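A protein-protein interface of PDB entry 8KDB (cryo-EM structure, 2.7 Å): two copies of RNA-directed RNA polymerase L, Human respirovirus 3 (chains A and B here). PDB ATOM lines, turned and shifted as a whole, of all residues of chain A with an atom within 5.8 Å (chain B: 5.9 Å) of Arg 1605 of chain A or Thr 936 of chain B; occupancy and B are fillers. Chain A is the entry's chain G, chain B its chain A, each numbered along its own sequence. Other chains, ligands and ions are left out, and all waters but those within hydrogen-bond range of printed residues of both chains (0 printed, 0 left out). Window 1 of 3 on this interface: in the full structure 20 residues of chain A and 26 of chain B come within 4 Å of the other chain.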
ATOM      1  N   TYR A1598     -24.138   1.424 -23.520  1.00  0.00           N
ATOM      2  CA  TYR A1598     -23.645   1.490 -22.149  1.00  0.00           C
ATOM      3  C   TYR A1598     -22.956   2.823 -21.870  1.00  0.00           C
ATOM      4  O   TYR A1598     -23.101   3.383 -20.775  1.00  0.00           O
ATOM      5  CB  TYR A1598     -22.700   0.331 -21.849  1.00  0.00           C
ATOM      6  CG  TYR A1598     -22.325   0.278 -20.388  1.00  0.00           C
ATOM      7  CD1 TYR A1598     -23.226  -0.186 -19.441  1.00  0.00           C
ATOM      8  CD2 TYR A1598     -21.082   0.714 -19.951  1.00  0.00           C
ATOM      9  CE1 TYR A1598     -22.898  -0.227 -18.103  1.00  0.00           C
ATOM     10  CE2 TYR A1598     -20.744   0.677 -18.614  1.00  0.00           C
ATOM     11  CZ  TYR A1598     -21.656   0.205 -17.694  1.00  0.00           C
ATOM     12  OH  TYR A1598     -21.325   0.164 -16.360  1.00  0.00           O
ATOM     13  N   LEU A1600     -23.445   5.868 -23.126  1.00  0.00           N
ATOM     14  CA  LEU A1600     -24.366   6.987 -22.936  1.00  0.00           C
ATOM     15  C   LEU A1600     -24.934   7.001 -21.522  1.00  0.00           C
ATOM     16  O   LEU A1600     -24.908   8.033 -20.836  1.00  0.00           O
ATOM     17  CB  LEU A1600     -25.495   6.912 -23.963  1.00  0.00           C
ATOM     18  CG  LEU A1600     -25.180   7.337 -25.396  1.00  0.00           C
ATOM     19  CD1 LEU A1600     -26.292   6.888 -26.328  1.00  0.00           C
ATOM     20  CD2 LEU A1600     -24.988   8.840 -25.478  1.00  0.00           C
ATOM     21  N   ASP A1601     -25.446   5.855 -21.067  1.00  0.00           N
ATOM     22  CA  ASP A1601     -26.026   5.773 -19.731  1.00  0.00           C
ATOM     23  C   ASP A1601     -24.979   6.037 -18.659  1.00  0.00           C
ATOM     24  O   ASP A1601     -25.252   6.737 -17.675  1.00  0.00           O
ATOM     25  CB  ASP A1601     -26.670   4.404 -19.523  1.00  0.00           C
ATOM     26  CG  ASP A1601     -28.103   4.353 -20.011  1.00  0.00           C
ATOM     27  OD1 ASP A1601     -28.674   5.428 -20.293  1.00  0.00           O
ATOM     28  OD2 ASP A1601     -28.658   3.241 -20.116  1.00  0.00           O
ATOM     29  N   LEU A1602     -23.775   5.483 -18.828  1.00  0.00           N
ATOM     30  CA  LEU A1602     -22.724   5.695 -17.840  1.00  0.00           C
ATOM     31  C   LEU A1602     -22.375   7.172 -17.722  1.00  0.00           C
ATOM     32  O   LEU A1602     -22.251   7.705 -16.611  1.00  0.00           O
ATOM     33  CB  LEU A1602     -21.488   4.877 -18.208  1.00  0.00           C
ATOM     34  CG  LEU A1602     -20.308   4.989 -17.243  1.00  0.00           C
ATOM     35  CD1 LEU A1602     -20.752   4.688 -15.822  1.00  0.00           C
ATOM     36  CD2 LEU A1602     -19.187   4.058 -17.664  1.00  0.00           C
ATOM     37  N   PHE A1603     -22.221   7.855 -18.859  1.00  0.00           N
ATOM     38  CA  PHE A1603     -21.881   9.271 -18.806  1.00  0.00           C
ATOM     39  C   PHE A1603     -23.003  10.087 -18.183  1.00  0.00           C
ATOM     40  O   PHE A1603     -22.744  11.014 -17.411  1.00  0.00           O
ATOM     41  CB  PHE A1603     -21.564   9.819 -20.194  1.00  0.00           C
ATOM     42  CG  PHE A1603     -21.482  11.316 -20.229  1.00  0.00           C
ATOM     43  CD1 PHE A1603     -20.445  11.975 -19.591  1.00  0.00           C
ATOM     44  CD2 PHE A1603     -22.460  12.068 -20.852  1.00  0.00           C
ATOM     45  CE1 PHE A1603     -20.368  13.350 -19.601  1.00  0.00           C
ATOM     46  CE2 PHE A1603     -22.389  13.445 -20.859  1.00  0.00           C
ATOM     47  CZ  PHE A1603     -21.341  14.086 -20.236  1.00  0.00           C
ATOM     48  N   MET A1604     -24.258   9.779 -18.527  1.00  0.00           N
ATOM     49  CA  MET A1604     -25.366  10.518 -17.929  1.00  0.00           C
ATOM     50  C   MET A1604     -25.390  10.343 -16.417  1.00  0.00           C
ATOM     51  O   MET A1604     -25.576  11.316 -15.674  1.00  0.00           O
ATOM     52  CB  MET A1604     -26.694  10.077 -18.537  1.00  0.00           C
ATOM     53  CG  MET A1604     -26.862  10.440 -19.994  1.00  0.00           C
ATOM     54  SD  MET A1604     -27.770  11.981 -20.187  1.00  0.00           S
ATOM     55  CE  MET A1604     -28.184  11.896 -21.921  1.00  0.00           C
ATOM     56  N   ARG A1605     -25.196   9.111 -15.942  1.00  0.00           N
ATOM     57  CA  ARG A1605     -25.194   8.867 -14.504  1.00  0.00           C
ATOM     58  C   ARG A1605     -24.055   9.618 -13.822  1.00  0.00           C
ATOM     59  O   ARG A1605     -24.252  10.257 -12.782  1.00  0.00           O
ATOM     60  CB  ARG A1605     -25.097   7.367 -14.231  1.00  0.00           C
ATOM     61  CG  ARG A1605     -25.199   6.997 -12.766  1.00  0.00           C
ATOM     62  CD  ARG A1605     -25.132   5.493 -12.575  1.00  0.00           C
ATOM     63  NE  ARG A1605     -26.268   4.818 -13.189  1.00  0.00           N
ATOM     64  CZ  ARG A1605     -26.183   4.011 -14.237  1.00  0.00           C
ATOM     65  NH1 ARG A1605     -25.020   3.734 -14.804  1.00  0.00           N
ATOM     66  NH2 ARG A1605     -27.292   3.465 -14.727  1.00  0.00           N
ATOM     67  N   GLU A1606     -22.853   9.562 -14.406  1.00  0.00           N
ATOM     68  CA  GLU A1606     -21.719  10.256 -13.803  1.00  0.00           C
ATOM     69  C   GLU A1606     -21.936  11.763 -13.774  1.00  0.00           C
ATOM     70  O   GLU A1606     -21.647  12.417 -12.766  1.00  0.00           O
ATOM     71  CB  GLU A1606     -20.429   9.916 -14.550  1.00  0.00           C
ATOM     72  CG  GLU A1606     -20.053   8.444 -14.516  1.00  0.00           C
ATOM     73  CD  GLU A1606     -19.595   7.979 -13.147  1.00  0.00           C
ATOM     74  OE1 GLU A1606     -19.377   8.831 -12.261  1.00  0.00           O
ATOM     75  OE2 GLU A1606     -19.451   6.753 -12.956  1.00  0.00           O
ATOM     76  N   TRP A1607     -22.442  12.333 -14.869  1.00  0.00           N
ATOM     77  CA  TRP A1607     -22.667  13.774 -14.912  1.00  0.00           C
ATOM     78  C   TRP A1607     -23.722  14.200 -13.902  1.00  0.00           C
ATOM     79  O   TRP A1607     -23.555  15.213 -13.211  1.00  0.00           O
ATOM     80  CB  TRP A1607     -23.071  14.207 -16.319  1.00  0.00           C
ATOM     81  CG  TRP A1607     -23.166  15.691 -16.462  1.00  0.00           C
ATOM     82  CD1 TRP A1607     -24.300  16.446 -16.415  1.00  0.00           C
ATOM     83  CD2 TRP A1607     -22.082  16.604 -16.653  1.00  0.00           C
ATOM     84  NE1 TRP A1607     -23.990  17.774 -16.576  1.00  0.00           N
ATOM     85  CE2 TRP A1607     -22.633  17.898 -16.723  1.00  0.00           C
ATOM     86  CE3 TRP A1607     -20.699  16.454 -16.775  1.00  0.00           C
ATOM     87  CZ2 TRP A1607     -21.850  19.033 -16.909  1.00  0.00           C
ATOM     88  CZ3 TRP A1607     -19.924  17.582 -16.961  1.00  0.00           C
ATOM     89  CH2 TRP A1607     -20.500  18.854 -17.025  1.00  0.00           C
ATOM     90  N   LEU A1608     -24.816  13.443 -13.795  1.00  0.00           N
ATOM     91  CA  LEU A1608     -25.847  13.791 -12.825  1.00  0.00           C
ATOM     92  C   LEU A1608     -25.378  13.594 -11.391  1.00  0.00           C
ATOM     93  O   LEU A1608     -25.892  14.263 -10.489  1.00  0.00           O
ATOM     94  CB  LEU A1608     -27.113  12.976 -13.087  1.00  0.00           C
ATOM     95  CG  LEU A1608     -27.872  13.362 -14.357  1.00  0.00           C
ATOM     96  CD1 LEU A1608     -29.189  12.617 -14.442  1.00  0.00           C
ATOM     97  CD2 LEU A1608     -28.098  14.864 -14.411  1.00  0.00           C
ATOM     98  N   ASN A1609     -24.418  12.701 -11.158  1.00  0.00           N
ATOM     99  CA  ASN A1609     -23.826  12.539  -9.838  1.00  0.00           C
ATOM    100  C   ASN A1609     -22.724  13.555  -9.555  1.00  0.00           C
ATOM    101  O   ASN A1609     -21.952  13.365  -8.610  1.00  0.00           O
ATOM    102  CB  ASN A1609     -23.280  11.118  -9.675  1.00  0.00           C
ATOM    103  CG  ASN A1609     -24.332  10.143  -9.191  1.00  0.00           C
ATOM    104  OD1 ASN A1609     -25.292  10.530  -8.526  1.00  0.00           O
ATOM    105  ND2 ASN A1609     -24.157   8.871  -9.522  1.00  0.00           N
ATOM    106  N   GLY A1610     -22.640  14.622 -10.343  1.00  0.00           N
ATOM    107  CA  GLY A1610     -21.666  15.676 -10.110  1.00  0.00           C
ATOM    108  C   GLY A1610     -20.215  15.290 -10.305  1.00  0.00           C
ATOM    109  O   GLY A1610     -19.368  15.652  -9.480  1.00  0.00           O
ATOM    110  N   TYR B  40     -31.652  -8.269  -7.965  1.00  0.00           N
ATOM    111  CA  TYR B  40     -31.460  -7.727  -6.635  1.00  0.00           C
ATOM    112  C   TYR B  40     -31.348  -8.848  -5.610  1.00  0.00           C
ATOM    113  O   TYR B  40     -31.980  -9.899  -5.759  1.00  0.00           O
ATOM    114  CB  TYR B  40     -32.617  -6.801  -6.244  1.00  0.00           C
ATOM    115  CG  TYR B  40     -32.487  -5.399  -6.785  1.00  0.00           C
ATOM    116  CD1 TYR B  40     -32.445  -5.164  -8.151  1.00  0.00           C
ATOM    117  CD2 TYR B  40     -32.406  -4.312  -5.930  1.00  0.00           C
ATOM    118  CE1 TYR B  40     -32.325  -3.886  -8.650  1.00  0.00           C
ATOM    119  CE2 TYR B  40     -32.286  -3.030  -6.420  1.00  0.00           C
ATOM    120  CZ  TYR B  40     -32.245  -2.823  -7.780  1.00  0.00           C
ATOM    121  OH  TYR B  40     -32.126  -1.545  -8.275  1.00  0.00           O
ATOM    122  N   ASN B 934     -30.041   0.849  -5.071  1.00  0.00           N
ATOM    123  CA  ASN B 934     -30.300   1.099  -6.483  1.00  0.00           C
ATOM    124  C   ASN B 934     -29.331   2.154  -7.000  1.00  0.00           C
ATOM    125  O   ASN B 934     -29.333   3.284  -6.496  1.00  0.00           O
ATOM    126  CB  ASN B 934     -31.743   1.550  -6.675  1.00  0.00           C
ATOM    127  CG  ASN B 934     -32.120   1.699  -8.130  1.00  0.00           C
ATOM    128  OD1 ASN B 934     -31.429   1.205  -9.018  1.00  0.00           O
ATOM    129  ND2 ASN B 934     -33.229   2.380  -8.384  1.00  0.00           N
ATOM    130  N   PRO B 935     -28.492   1.842  -7.993  1.00  0.00           N
ATOM    131  CA  PRO B 935     -27.493   2.816  -8.450  1.00  0.00           C
ATOM    132  C   PRO B 935     -28.021   3.851  -9.430  1.00  0.00           C
ATOM    133  O   PRO B 935     -27.292   4.800  -9.744  1.00  0.00           O
ATOM    134  CB  PRO B 935     -26.436   1.929  -9.115  1.00  0.00           C
ATOM    135  CG  PRO B 935     -27.219   0.779  -9.637  1.00  0.00           C
ATOM    136  CD  PRO B 935     -28.315   0.529  -8.636  1.00  0.00           C
ATOM    137  N   THR B 936     -29.251   3.707  -9.923  1.00  0.00           N
ATOM    138  CA  THR B 936     -29.777   4.652 -10.899  1.00  0.00           C
ATOM    139  C   THR B 936     -30.287   5.938 -10.263  1.00  0.00           C
ATOM    140  O   THR B 936     -30.502   6.921 -10.980  1.00  0.00           O
ATOM    141  CB  THR B 936     -30.900   4.006 -11.711  1.00  0.00           C
ATOM    142  OG1 THR B 936     -31.946   3.580 -10.830  1.00  0.00           O
ATOM    143  CG2 THR B 936     -30.377   2.807 -12.480  1.00  0.00           C
ATOM    144  N   ILE B 937     -30.486   5.957  -8.949  1.00  0.00           N
ATOM    145  CA  ILE B 937     -30.944   7.166  -8.267  1.00  0.00           C
ATOM    146  C   ILE B 937     -29.773   8.142  -8.200  1.00  0.00           C
ATOM    147  O   ILE B 937     -28.809   7.921  -7.463  1.00  0.00           O
ATOM    148  CB  ILE B 937     -31.491   6.854  -6.871  1.00  0.00           C
ATOM    149  CG1 ILE B 937     -32.637   5.847  -6.960  1.00  0.00           C
ATOM    150  CG2 ILE B 937     -31.967   8.126  -6.194  1.00  0.00           C
ATOM    151  CD1 ILE B 937     -33.842   6.360  -7.707  1.00  0.00           C
ATOM    152  N   THR B 938     -29.858   9.224  -8.966  1.00  0.00           N
ATOM    153  CA  THR B 938     -28.770  10.185  -9.069  1.00  0.00           C
ATOM    154  C   THR B 938     -28.825  11.159  -7.893  1.00  0.00           C
ATOM    155  O   THR B 938     -29.591  10.986  -6.941  1.00  0.00           O
ATOM    156  CB  THR B 938     -28.833  10.910 -10.411  1.00  0.00           C
ATOM    157  OG1 THR B 938     -30.121  11.519 -10.563  1.00  0.00           O
ATOM    158  CG2 THR B 938     -28.609   9.931 -11.549  1.00  0.00           C
ATOM    159  N   SER B1129     -34.890  -1.444 -15.289  1.00  0.00           N
ATOM    160  CA  SER B1129     -33.878  -0.926 -14.377  1.00  0.00           C
ATOM    161  C   SER B1129     -34.024   0.566 -14.101  1.00  0.00           C
ATOM    162  O   SER B1129     -33.474   1.042 -13.104  1.00  0.00           O
ATOM    163  CB  SER B1129     -32.479  -1.215 -14.922  1.00  0.00           C
ATOM    164  OG  SER B1129     -32.154  -0.349 -15.992  1.00  0.00           O
ATOM    165  N   ASN B1130     -34.743   1.310 -14.942  1.00  0.00           N
ATOM    166  CA  ASN B1130     -34.922   2.743 -14.730  1.00  0.00           C
ATOM    167  C   ASN B1130     -36.285   3.106 -14.140  1.00  0.00           C
ATOM    168  O   ASN B1130     -36.638   4.291 -14.117  1.00  0.00           O
ATOM    169  CB  ASN B1130     -34.712   3.496 -16.044  1.00  0.00           C
ATOM    170  CG  ASN B1130     -33.251   3.636 -16.404  1.00  0.00           C
ATOM    171  OD1 ASN B1130     -32.373   3.442 -15.567  1.00  0.00           O
ATOM    172  ND2 ASN B1130     -32.980   3.975 -17.657  1.00  0.00           N
ATOM    173  N   ASP B1132     -37.944   3.139 -11.056  1.00  0.00           N
ATOM    174  CA  ASP B1132     -38.138   4.003  -9.896  1.00  0.00           C
ATOM    175  C   ASP B1132     -37.668   5.424 -10.182  1.00  0.00           C
ATOM    176  O   ASP B1132     -38.325   6.401  -9.789  1.00  0.00           O
ATOM    177  CB  ASP B1132     -37.402   3.422  -8.690  1.00  0.00           C
ATOM    178  CG  ASP B1132     -38.135   3.663  -7.388  1.00  0.00           C
ATOM    179  OD1 ASP B1132     -39.346   3.961  -7.434  1.00  0.00           O
ATOM    180  OD2 ASP B1132     -37.501   3.554  -6.318  1.00  0.00           O
ATOM    181  N   LEU B1133     -36.532   5.554 -10.868  1.00  0.00           N
ATOM    182  CA  LEU B1133     -36.030   6.872 -11.226  1.00  0.00           C
ATOM    183  C   LEU B1133     -37.011   7.601 -12.134  1.00  0.00           C
ATOM    184  O   LEU B1133     -37.235   8.806 -11.974  1.00  0.00           O
ATOM    185  CB  LEU B1133     -34.662   6.745 -11.893  1.00  0.00           C
ATOM    186  CG  LEU B1133     -34.081   8.018 -12.501  1.00  0.00           C
ATOM    187  CD1 LEU B1133     -33.639   8.968 -11.404  1.00  0.00           C
ATOM    188  CD2 LEU B1133     -32.928   7.688 -13.429  1.00  0.00           C
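ND2 of Asn 934 of chain B lies within hydrogen-bond range of OG1 of Thr 936 of chain B, 3.0 Å away.
Among the printed residues, pairs that only touch across the chains: Arg 1605 of chain A with Pro 935 of chain B, Arg 1605 of chain A with Thr 936 of chain B, Leu 1608 of chain A with Thr 938 of chain B and Asn 1609 of chain A with Thr 938 of chain B.
Of chain B, only Pro 935 (3.6 Å) and Thr 936 (3.9 Å) come within 4 Å of Arg 1605 of chain A. Thr 936 of chain B touches one residue of chain A. Of the printed residues of chain A, Thr 938 of chain B touches Leu 1608 (3.7 Å) and Asn 1609 (3.5 Å). Of the printed residues of chain B, Asn 1609 of chain A touches Thr 938. Of the printed residues of chain B, Leu 1608 of chain A touches Thr 938. Printed residues of chain A within 4 Å of Pro 935 of chain B: Arg 1605 (3.6 Å). The nearest printed residue of chain A that does not touch Thr 936 of chain B is Leu 1608 of chain A (6.8 Å). The nearest printed residue of chain A that does not touch Thr 938 of chain B is Arg 1605 of chain A (4.5 Å).
Of the 12 printed residues of chain A, 3 touch a printed residue of chain B. Hydrophobic or aromatic side chains of chain A within 4 Å of the printed part of chain B: Leu 1608. Along chain B the printed residues that touch a printed residue of chain A span positions 935 to 938. Among the printed residues, 4 pairs touch across the chains. Among the printed residues, no Asp or Glu carboxylate lies within 4 Å of a Lys or Arg side-chain nitrogen of the other chain.
No position is printed for both chains. Of the 4 pairs that touch across the chains among the printed residues, none has its exchanged pair printed and touching as well.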
